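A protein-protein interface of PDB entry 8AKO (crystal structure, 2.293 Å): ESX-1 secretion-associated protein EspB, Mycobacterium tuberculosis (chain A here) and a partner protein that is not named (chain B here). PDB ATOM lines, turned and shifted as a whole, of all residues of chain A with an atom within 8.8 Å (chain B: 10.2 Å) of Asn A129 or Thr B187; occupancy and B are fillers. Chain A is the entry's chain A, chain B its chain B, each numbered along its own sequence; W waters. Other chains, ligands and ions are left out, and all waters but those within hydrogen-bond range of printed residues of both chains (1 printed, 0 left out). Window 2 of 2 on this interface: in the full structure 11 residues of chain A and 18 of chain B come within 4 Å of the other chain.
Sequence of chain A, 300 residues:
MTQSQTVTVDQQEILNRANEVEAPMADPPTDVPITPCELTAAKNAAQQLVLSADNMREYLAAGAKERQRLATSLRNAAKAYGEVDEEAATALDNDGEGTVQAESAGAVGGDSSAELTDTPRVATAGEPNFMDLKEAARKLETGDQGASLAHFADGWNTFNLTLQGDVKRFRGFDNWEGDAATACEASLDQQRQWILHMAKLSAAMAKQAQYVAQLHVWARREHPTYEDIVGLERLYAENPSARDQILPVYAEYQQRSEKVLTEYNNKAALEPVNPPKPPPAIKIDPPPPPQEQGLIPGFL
NE2 of Gln A254 is in hydrogen-bond range of OE2 of Glu A258 (3.2 Å). The backbone carbonyl oxygen (O) of Glu A258 is in hydrogen-bond range of the side-chain hydroxyl (OG1) of Thr A262, at 3.2 Å. The guanidinium group (NH1) of Arg B189 sits at hydrogen-bond distance from the side-chain hydroxyl (OG1) of Thr B78, at 2.9 Å. The backbone NH (N) of Ala B186 is in hydrogen-bond range of the side-chain hydroxyl (OG) of Ser B184, 3.2 Å away. The guanidinium group of Arg B189 is in hydrogen-bond range of the backbone carbonyl oxygen of Ser B184, at 3.2 Å. The backbone NH of Gly B188 lies within hydrogen-bond range of the side-chain carboxylate of Glu B190 (3.3 Å).
Among the printed residues, merely in contact across the chains: Asn A129 with Thr B187, Phe A130 with Ser B184, Phe A130 with Ala B186, Phe A130 with Arg B189, Phe A130 with Gly B188, Phe A130 with Ala B192 and Phe A130 with Pro B181.
The backbone NH of Phe A130 lies within hydrogen-bond range of the backbone carbonyl oxygen of Thr B187 (2.9 Å). OE2 of Glu A258 is in hydrogen-bond range of OG of Ser B184, at 2.6 Å.
Printed residues of chain B that touch a printed residue of chain A: Pro B181, Ser B184, Ala B186, Thr B187, Gly B188, Arg B189 and Ala B192. Hydrophobic or aromatic side chains of chain B within 4 Å of the printed part of chain A: Pro B181, Ala B186 and Ala B192. Along chain A the printed residues that touch a printed residue of chain B span positions 129 to 258. Among the printed residues, 9 pairs touch across the chains.
Water W1 bridges the side-chain hydroxyl (OG1) of Thr B185 (2.6 Å) and the side-chain carboxylate (OE1) of Glu A258 (3.2 Å).
Asn A129 touches just one residue of chain B: Thr B187 (3.4 Å). Of chain A, only Asn A129 (3.4 Å) and Phe A130 (2.9 Å) come within 4 Å of Thr B187. Of the printed residues of chain A, Pro B181 touches Phe A130. Printed residues of chain B within 4 Å of Phe A130: Pro B181, Ser B184, Ala B186, Thr B187, Gly B188, Arg B189 and Ala B192. Of the printed residues of chain A, Arg B189 touches Phe A130 (3.7 Å). Of the printed residues of chain B, Glu A258 touches Ser B184. Of the printed residues of chain A, Ser B184 touches Phe A130 (3.6 Å) and Glu A258 (2.6 Å). The nearest residue of chain B that does not touch Asn A129 is Ala B186 (4.3 Å). The nearest residue of chain A that does not touch Thr B187 is Pro A128 (4.9 Å).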
ATOM      1  N   ALA A 125      22.769 -10.916  43.083  1.00  0.00           N
ATOM      2  CA  ALA A 125      22.820 -10.877  41.630  1.00  0.00           C
ATOM      3  C   ALA A 125      22.748  -9.444  41.146  1.00  0.00           C
ATOM      4  O   ALA A 125      22.197  -8.583  41.828  1.00  0.00           O
ATOM      5  CB  ALA A 125      21.678 -11.651  41.022  1.00  0.00           C
ATOM      6  N   GLY A 126      23.286  -9.220  39.939  1.00  0.00           N
ATOM      7  CA  GLY A 126      23.264  -7.901  39.330  1.00  0.00           C
ATOM      8  C   GLY A 126      21.958  -7.658  38.572  1.00  0.00           C
ATOM      9  O   GLY A 126      20.857  -7.838  39.110  1.00  0.00           O
ATOM     10  N   GLU A 127      22.088  -7.206  37.319  1.00  0.00           N
ATOM     11  CA  GLU A 127      20.918  -7.139  36.464  1.00  0.00           C
ATOM     12  C   GLU A 127      20.514  -8.569  36.166  1.00  0.00           C
ATOM     13  O   GLU A 127      21.360  -9.406  35.879  1.00  0.00           O
ATOM     14  CB  GLU A 127      21.222  -6.414  35.167  1.00  0.00           C
ATOM     15  CG  GLU A 127      21.558  -4.958  35.369  1.00  0.00           C
ATOM     16  CD  GLU A 127      21.411  -4.185  34.068  1.00  0.00           C
ATOM     17  OE1 GLU A 127      21.936  -4.673  33.036  1.00  0.00           O
ATOM     18  OE2 GLU A 127      20.760  -3.108  34.080  1.00  0.00           O
ATOM     19  N   PRO A 128      19.215  -8.912  36.241  1.00  0.00           N
ATOM     20  CA  PRO A 128      18.817 -10.318  36.147  1.00  0.00           C
ATOM     21  C   PRO A 128      18.824 -10.816  34.701  1.00  0.00           C
ATOM     22  O   PRO A 128      18.738 -10.049  33.742  1.00  0.00           O
ATOM     23  CB  PRO A 128      17.390 -10.307  36.688  1.00  0.00           C
ATOM     24  CG  PRO A 128      16.880  -8.908  36.371  1.00  0.00           C
ATOM     25  CD  PRO A 128      18.079  -7.980  36.337  1.00  0.00           C
ATOM     26  N   ASN A 129      18.941 -12.130  34.566  1.00  0.00           N
ATOM     27  CA  ASN A 129      18.885 -12.757  33.264  1.00  0.00           C
ATOM     28  C   ASN A 129      17.428 -12.870  32.843  1.00  0.00           C
ATOM     29  O   ASN A 129      16.561 -12.640  33.669  1.00  0.00           O
ATOM     30  CB  ASN A 129      19.491 -14.156  33.327  1.00  0.00           C
ATOM     31  CG  ASN A 129      20.998 -14.107  33.264  1.00  0.00           C
ATOM     32  OD1 ASN A 129      21.576 -13.096  32.837  1.00  0.00           O
ATOM     33  ND2 ASN A 129      21.617 -15.192  33.701  1.00  0.00           N
ATOM     34  N   PHE A 130      17.181 -13.235  31.575  1.00  0.00           N
ATOM     35  CA  PHE A 130      15.840 -13.467  31.076  1.00  0.00           C
ATOM     36  C   PHE A 130      15.088 -14.481  31.943  1.00  0.00           C
ATOM     37  O   PHE A 130      15.618 -15.508  32.344  1.00  0.00           O
ATOM     38  CB  PHE A 130      15.892 -13.908  29.611  1.00  0.00           C
ATOM     39  CG  PHE A 130      14.547 -14.336  29.072  1.00  0.00           C
ATOM     40  CD1 PHE A 130      13.608 -13.378  28.722  1.00  0.00           C
ATOM     41  CD2 PHE A 130      14.196 -15.681  28.974  1.00  0.00           C
ATOM     42  CE1 PHE A 130      12.360 -13.746  28.256  1.00  0.00           C
ATOM     43  CE2 PHE A 130      12.935 -16.055  28.523  1.00  0.00           C
ATOM     44  CZ  PHE A 130      12.027 -15.083  28.145  1.00  0.00           C
ATOM     45  N   MET A 131      13.815 -14.197  32.206  1.00  0.00           N
ATOM     46  CA  MET A 131      12.959 -15.140  32.899  1.00  0.00           C
ATOM     47  C   MET A 131      11.587 -15.144  32.238  1.00  0.00           C
ATOM     48  O   MET A 131      11.107 -14.092  31.812  1.00  0.00           O
ATOM     49  CB  MET A 131      12.786 -14.694  34.344  1.00  0.00           C
ATOM     50  CG  MET A 131      12.470 -15.842  35.213  1.00  0.00           C
ATOM     51  SD  MET A 131      11.977 -15.353  36.857  1.00  0.00           S
ATOM     52  CE  MET A 131      12.399 -16.835  37.758  1.00  0.00           C
ATOM     53  N   ASP A 132      10.972 -16.334  32.181  1.00  0.00           N
ATOM     54  CA  ASP A 132       9.634 -16.495  31.631  1.00  0.00           C
ATOM     55  C   ASP A 132       8.645 -15.720  32.487  1.00  0.00           C
ATOM     56  O   ASP A 132       8.724 -15.760  33.714  1.00  0.00           O
ATOM     57  CB  ASP A 132       9.221 -17.969  31.598  1.00  0.00           C
ATOM     58  CG  ASP A 132       7.807 -18.202  31.094  1.00  0.00           C
ATOM     59  OD1 ASP A 132       7.131 -19.086  31.674  1.00  0.00           O
ATOM     60  OD2 ASP A 132       7.389 -17.503  30.128  1.00  0.00           O
ATOM     61  N   ALA A 136       7.992 -15.913  36.499  1.00  0.00           N
ATOM     62  CA  ALA A 136       8.238 -14.777  37.381  1.00  0.00           C
ATOM     63  C   ALA A 136       6.981 -14.430  38.170  1.00  0.00           C
ATOM     64  O   ALA A 136       7.042 -14.096  39.344  1.00  0.00           O
ATOM     65  CB  ALA A 136       8.703 -13.579  36.581  1.00  0.00           C
ATOM     66  N   GLN A 254       5.981  -8.090  29.332  1.00  0.00           N
ATOM     67  CA  GLN A 254       7.331  -8.553  29.604  1.00  0.00           C
ATOM     68  C   GLN A 254       8.118  -7.407  30.224  1.00  0.00           C
ATOM     69  O   GLN A 254       8.796  -7.609  31.228  1.00  0.00           O
ATOM     70  CB  GLN A 254       8.018  -9.045  28.329  1.00  0.00           C
ATOM     71  CG  GLN A 254       9.404  -9.644  28.496  1.00  0.00           C
ATOM     72  CD  GLN A 254       9.372 -11.053  29.043  1.00  0.00           C
ATOM     73  OE1 GLN A 254       8.427 -11.818  28.825  1.00  0.00           O
ATOM     74  NE2 GLN A 254      10.424 -11.415  29.765  1.00  0.00           N
ATOM     75  N   SER A 257       7.742  -6.488  33.859  1.00  0.00           N
ATOM     76  CA  SER A 257       8.127  -7.597  34.714  1.00  0.00           C
ATOM     77  C   SER A 257       9.608  -7.526  35.016  1.00  0.00           C
ATOM     78  O   SER A 257      10.123  -7.633  36.107  1.00  0.00           O
ATOM     79  CB  SER A 257       7.813  -8.881  34.030  1.00  0.00           C
ATOM     80  OG  SER A 257       8.448  -9.945  34.700  1.00  0.00           O
ATOM     81  N   GLU A 258      10.286  -7.366  33.970  1.00  0.00           N
ATOM     82  CA  GLU A 258      11.635  -6.970  33.919  1.00  0.00           C
ATOM     83  C   GLU A 258      11.965  -5.666  34.579  1.00  0.00           C
ATOM     84  O   GLU A 258      12.980  -5.671  35.190  1.00  0.00           O
ATOM     85  CB  GLU A 258      11.972  -6.857  32.463  1.00  0.00           C
ATOM     86  CG  GLU A 258      12.487  -8.151  31.976  1.00  0.00           C
ATOM     87  CD  GLU A 258      12.868  -8.184  30.504  1.00  0.00           C
ATOM     88  OE1 GLU A 258      13.240  -7.132  29.972  1.00  0.00           O
ATOM     89  OE2 GLU A 258      12.747  -9.284  29.868  1.00  0.00           O
ATOM     90  N   LEU A 261      11.788  -6.982  38.292  1.00  0.00           N
ATOM     91  CA  LEU A 261      12.869  -7.883  38.642  1.00  0.00           C
ATOM     92  C   LEU A 261      14.184  -7.121  38.778  1.00  0.00           C
ATOM     93  O   LEU A 261      14.904  -7.369  39.731  1.00  0.00           O
ATOM     94  CB  LEU A 261      12.924  -9.018  37.625  1.00  0.00           C
ATOM     95  CG  LEU A 261      12.130 -10.271  37.994  1.00  0.00           C
ATOM     96  CD1 LEU A 261      10.653 -10.013  38.209  1.00  0.00           C
ATOM     97  CD2 LEU A 261      12.260 -11.254  36.857  1.00  0.00           C
ATOM     98  N   THR A 262      14.439  -6.120  37.931  1.00  0.00           N
ATOM     99  CA  THR A 262      15.671  -5.353  38.045  1.00  0.00           C
ATOM    100  C   THR A 262      15.705  -4.601  39.368  1.00  0.00           C
ATOM    101  O   THR A 262      16.719  -4.639  40.066  1.00  0.00           O
ATOM    102  CB  THR A 262      15.890  -4.376  36.880  1.00  0.00           C
ATOM    103  OG1 THR A 262      16.080  -5.159  35.705  1.00  0.00           O
ATOM    104  CG2 THR A 262      17.111  -3.493  37.045  1.00  0.00           C
ATOM    105  N   ASN A 265      16.069  -6.898  42.300  1.00  0.00           N
ATOM    106  CA  ASN A 265      17.442  -7.377  42.457  1.00  0.00           C
ATOM    107  C   ASN A 265      18.296  -6.288  43.067  1.00  0.00           C
ATOM    108  O   ASN A 265      19.243  -6.602  43.765  1.00  0.00           O
ATOM    109  CB  ASN A 265      18.114  -7.835  41.169  1.00  0.00           C
ATOM    110  CG  ASN A 265      17.858  -9.300  40.942  1.00  0.00           C
ATOM    111  OD1 ASN A 265      17.049  -9.903  41.650  1.00  0.00           O
ATOM    112  ND2 ASN A 265      18.539  -9.874  39.960  1.00  0.00           N
ATOM    113  N   THR B  78      19.836 -14.561  16.512  1.00  0.00           N
ATOM    114  CA  THR B  78      18.801 -13.527  16.565  1.00  0.00           C
ATOM    115  C   THR B  78      19.333 -12.113  16.288  1.00  0.00           C
ATOM    116  O   THR B  78      18.570 -11.157  16.358  1.00  0.00           O
ATOM    117  CB  THR B  78      17.951 -13.548  17.852  1.00  0.00           C
ATOM    118  OG1 THR B  78      18.735 -13.033  18.931  1.00  0.00           O
ATOM    119  CG2 THR B  78      17.347 -14.899  18.202  1.00  0.00           C
ATOM    120  N   TYR B  79      20.633 -11.965  16.010  1.00  0.00           N
ATOM    121  CA  TYR B  79      21.245 -10.668  15.747  1.00  0.00           C
ATOM    122  C   TYR B  79      21.856 -10.728  14.347  1.00  0.00           C
ATOM    123  O   TYR B  79      23.036 -11.056  14.213  1.00  0.00           O
ATOM    124  CB  TYR B  79      22.345 -10.351  16.775  1.00  0.00           C
ATOM    125  CG  TYR B  79      21.984 -10.149  18.234  1.00  0.00           C
ATOM    126  CD1 TYR B  79      22.885  -9.540  19.095  1.00  0.00           C
ATOM    127  CD2 TYR B  79      20.773 -10.563  18.782  1.00  0.00           C
ATOM    128  CE1 TYR B  79      22.605  -9.360  20.446  1.00  0.00           C
ATOM    129  CE2 TYR B  79      20.477 -10.398  20.127  1.00  0.00           C
ATOM    130  CZ  TYR B  79      21.394  -9.792  20.965  1.00  0.00           C
ATOM    131  OH  TYR B  79      21.088  -9.617  22.281  1.00  0.00           O
ATOM    132  N   PRO B 181      10.594 -14.995  24.005  1.00  0.00           N
ATOM    133  CA  PRO B 181      11.810 -14.262  24.364  1.00  0.00           C
ATOM    134  C   PRO B 181      12.211 -13.135  23.427  1.00  0.00           C
ATOM    135  O   PRO B 181      13.107 -12.357  23.766  1.00  0.00           O
ATOM    136  CB  PRO B 181      12.909 -15.325  24.389  1.00  0.00           C
ATOM    137  CG  PRO B 181      12.153 -16.627  24.493  1.00  0.00           C
ATOM    138  CD  PRO B 181      10.902 -16.405  23.685  1.00  0.00           C
ATOM    139  N   SER B 184      12.038  -9.430  24.514  1.00  0.00           N
ATOM    140  CA  SER B 184      12.941  -9.108  25.610  1.00  0.00           C
ATOM    141  C   SER B 184      14.311  -8.774  25.044  1.00  0.00           C
ATOM    142  O   SER B 184      14.644  -9.212  23.949  1.00  0.00           O
ATOM    143  CB  SER B 184      13.012 -10.256  26.600  1.00  0.00           C
ATOM    144  OG  SER B 184      13.913  -9.959  27.654  1.00  0.00           O
ATOM    145  N   THR B 185      15.103  -8.016  25.807  1.00  0.00           N
ATOM    146  CA  THR B 185      16.490  -7.779  25.429  1.00  0.00           C
ATOM    147  C   THR B 185      17.416  -8.136  26.589  1.00  0.00           C
ATOM    148  O   THR B 185      18.588  -7.742  26.600  1.00  0.00           O
ATOM    149  CB  THR B 185      16.765  -6.333  24.996  1.00  0.00           C
ATOM    150  OG1 THR B 185      16.081  -5.470  25.904  1.00  0.00           O
ATOM    151  CG2 THR B 185      16.380  -6.057  23.563  1.00  0.00           C
ATOM    152  N   ALA B 186      16.880  -8.884  27.561  1.00  0.00           N
ATOM    153  CA  ALA B 186      17.667  -9.402  28.676  1.00  0.00           C
ATOM    154  C   ALA B 186      18.738 -10.381  28.182  1.00  0.00           C
ATOM    155  O   ALA B 186      18.601 -10.995  27.131  1.00  0.00           O
ATOM    156  CB  ALA B 186      16.747 -10.066  29.681  1.00  0.00           C
ATOM    157  N   THR B 187      19.815 -10.538  28.950  1.00  0.00           N
ATOM    158  CA  THR B 187      20.801 -11.580  28.723  1.00  0.00           C
ATOM    159  C   THR B 187      20.154 -12.952  28.900  1.00  0.00           C
ATOM    160  O   THR B 187      19.542 -13.226  29.924  1.00  0.00           O
ATOM    161  CB  THR B 187      21.928 -11.429  29.745  1.00  0.00           C
ATOM    162  OG1 THR B 187      22.633 -10.261  29.333  1.00  0.00           O
ATOM    163  CG2 THR B 187      22.864 -12.611  29.764  1.00  0.00           C
ATOM    164  N   GLY B 188      20.249 -13.798  27.873  1.00  0.00           N
ATOM    165  CA  GLY B 188      19.716 -15.148  27.949  1.00  0.00           C
ATOM    166  C   GLY B 188      18.412 -15.343  27.181  1.00  0.00           C
ATOM    167  O   GLY B 188      17.849 -16.441  27.203  1.00  0.00           O
ATOM    168  N   ARG B 189      17.914 -14.298  26.500  1.00  0.00           N
ATOM    169  CA  ARG B 189      16.707 -14.501  25.710  1.00  0.00           C
ATOM    170  C   ARG B 189      17.006 -15.297  24.444  1.00  0.00           C
ATOM    171  O   ARG B 189      16.132 -16.036  23.965  1.00  0.00           O
ATOM    172  CB  ARG B 189      16.000 -13.189  25.388  1.00  0.00           C
ATOM    173  CG  ARG B 189      16.835 -12.153  24.654  1.00  0.00           C
ATOM    174  CD  ARG B 189      16.520 -12.130  23.170  1.00  0.00           C
ATOM    175  NE  ARG B 189      16.929 -10.884  22.545  1.00  0.00           N
ATOM    176  CZ  ARG B 189      16.968 -10.680  21.237  1.00  0.00           C
ATOM    177  NH1 ARG B 189      16.641 -11.653  20.409  1.00  0.00           N
ATOM    178  NH2 ARG B 189      17.342  -9.510  20.760  1.00  0.00           N
ATOM    179  N   GLU B 190      18.245 -15.137  23.943  1.00  0.00           N
ATOM    180  CA  GLU B 190      18.724 -15.837  22.758  1.00  0.00           C
ATOM    181  C   GLU B 190      18.612 -17.352  22.958  1.00  0.00           C
ATOM    182  O   GLU B 190      18.053 -18.062  22.120  1.00  0.00           O
ATOM    183  CB  GLU B 190      20.143 -15.385  22.400  1.00  0.00           C
ATOM    184  CG  GLU B 190      20.350 -13.873  22.354  1.00  0.00           C
ATOM    185  CD  GLU B 190      20.829 -13.240  23.649  1.00  0.00           C
ATOM    186  OE1 GLU B 190      21.016 -13.976  24.643  1.00  0.00           O
ATOM    187  OE2 GLU B 190      21.021 -12.019  23.664  1.00  0.00           O
ATOM    188  N   ALA B 191      19.117 -17.833  24.098  1.00  0.00           N
ATOM    189  CA  ALA B 191      19.142 -19.254  24.363  1.00  0.00           C
ATOM    190  C   ALA B 191      17.733 -19.812  24.513  1.00  0.00           C
ATOM    191  O   ALA B 191      17.483 -20.923  24.062  1.00  0.00           O
ATOM    192  CB  ALA B 191      19.975 -19.517  25.583  1.00  0.00           C
ATOM    193  N   ALA B 192      16.833 -19.054  25.159  1.00  0.00           N
ATOM    194  CA  ALA B 192      15.470 -19.514  25.400  1.00  0.00           C
ATOM    195  C   ALA B 192      14.688 -19.565  24.088  1.00  0.00           C
ATOM    196  O   ALA B 192      13.847 -20.457  23.892  1.00  0.00           O
ATOM    197  CB  ALA B 192      14.798 -18.625  26.415  1.00  0.00           C
ATOM    198  N   HIS B 193      15.012 -18.616  23.199  1.00  0.00           N
ATOM    199  CA  HIS B 193      14.442 -18.613  21.860  1.00  0.00           C
ATOM    200  C   HIS B 193      14.896 -19.842  21.074  1.00  0.00           C
ATOM    201  O   HIS B 193      14.090 -20.477  20.385  1.00  0.00           O
ATOM    202  CB  HIS B 193      14.794 -17.310  21.129  1.00  0.00           C
ATOM    203  CG  HIS B 193      14.415 -17.330  19.681  1.00  0.00           C
ATOM    204  ND1 HIS B 193      13.108 -17.192  19.251  1.00  0.00           N
ATOM    205  CD2 HIS B 193      15.170 -17.487  18.575  1.00  0.00           C
ATOM    206  CE1 HIS B 193      13.086 -17.261  17.939  1.00  0.00           C
ATOM    207  NE2 HIS B 193      14.333 -17.453  17.503  1.00  0.00           N
ATOM    208  N   ARG B 195      15.812 -22.734  22.342  1.00  0.00           N
ATOM    209  CA  ARG B 195      15.214 -23.945  22.884  1.00  0.00           C
ATOM    210  C   ARG B 195      13.789 -24.118  22.368  1.00  0.00           C
ATOM    211  O   ARG B 195      13.379 -25.237  22.059  1.00  0.00           O
ATOM    212  CB  ARG B 195      15.190 -23.916  24.412  1.00  0.00           C
ATOM    213  CG  ARG B 195      16.564 -23.906  25.052  1.00  0.00           C
ATOM    214  CD  ARG B 195      16.420 -24.101  26.546  1.00  0.00           C
ATOM    215  NE  ARG B 195      17.350 -23.219  27.249  1.00  0.00           N
ATOM    216  CZ  ARG B 195      17.006 -22.105  27.900  1.00  0.00           C
ATOM    217  NH1 ARG B 195      15.735 -21.730  27.969  1.00  0.00           N
ATOM    218  NH2 ARG B 195      17.942 -21.378  28.490  1.00  0.00           N
HETATM  219  O   HOH W   1      13.955  -5.420  27.417  1.00  0.00           O
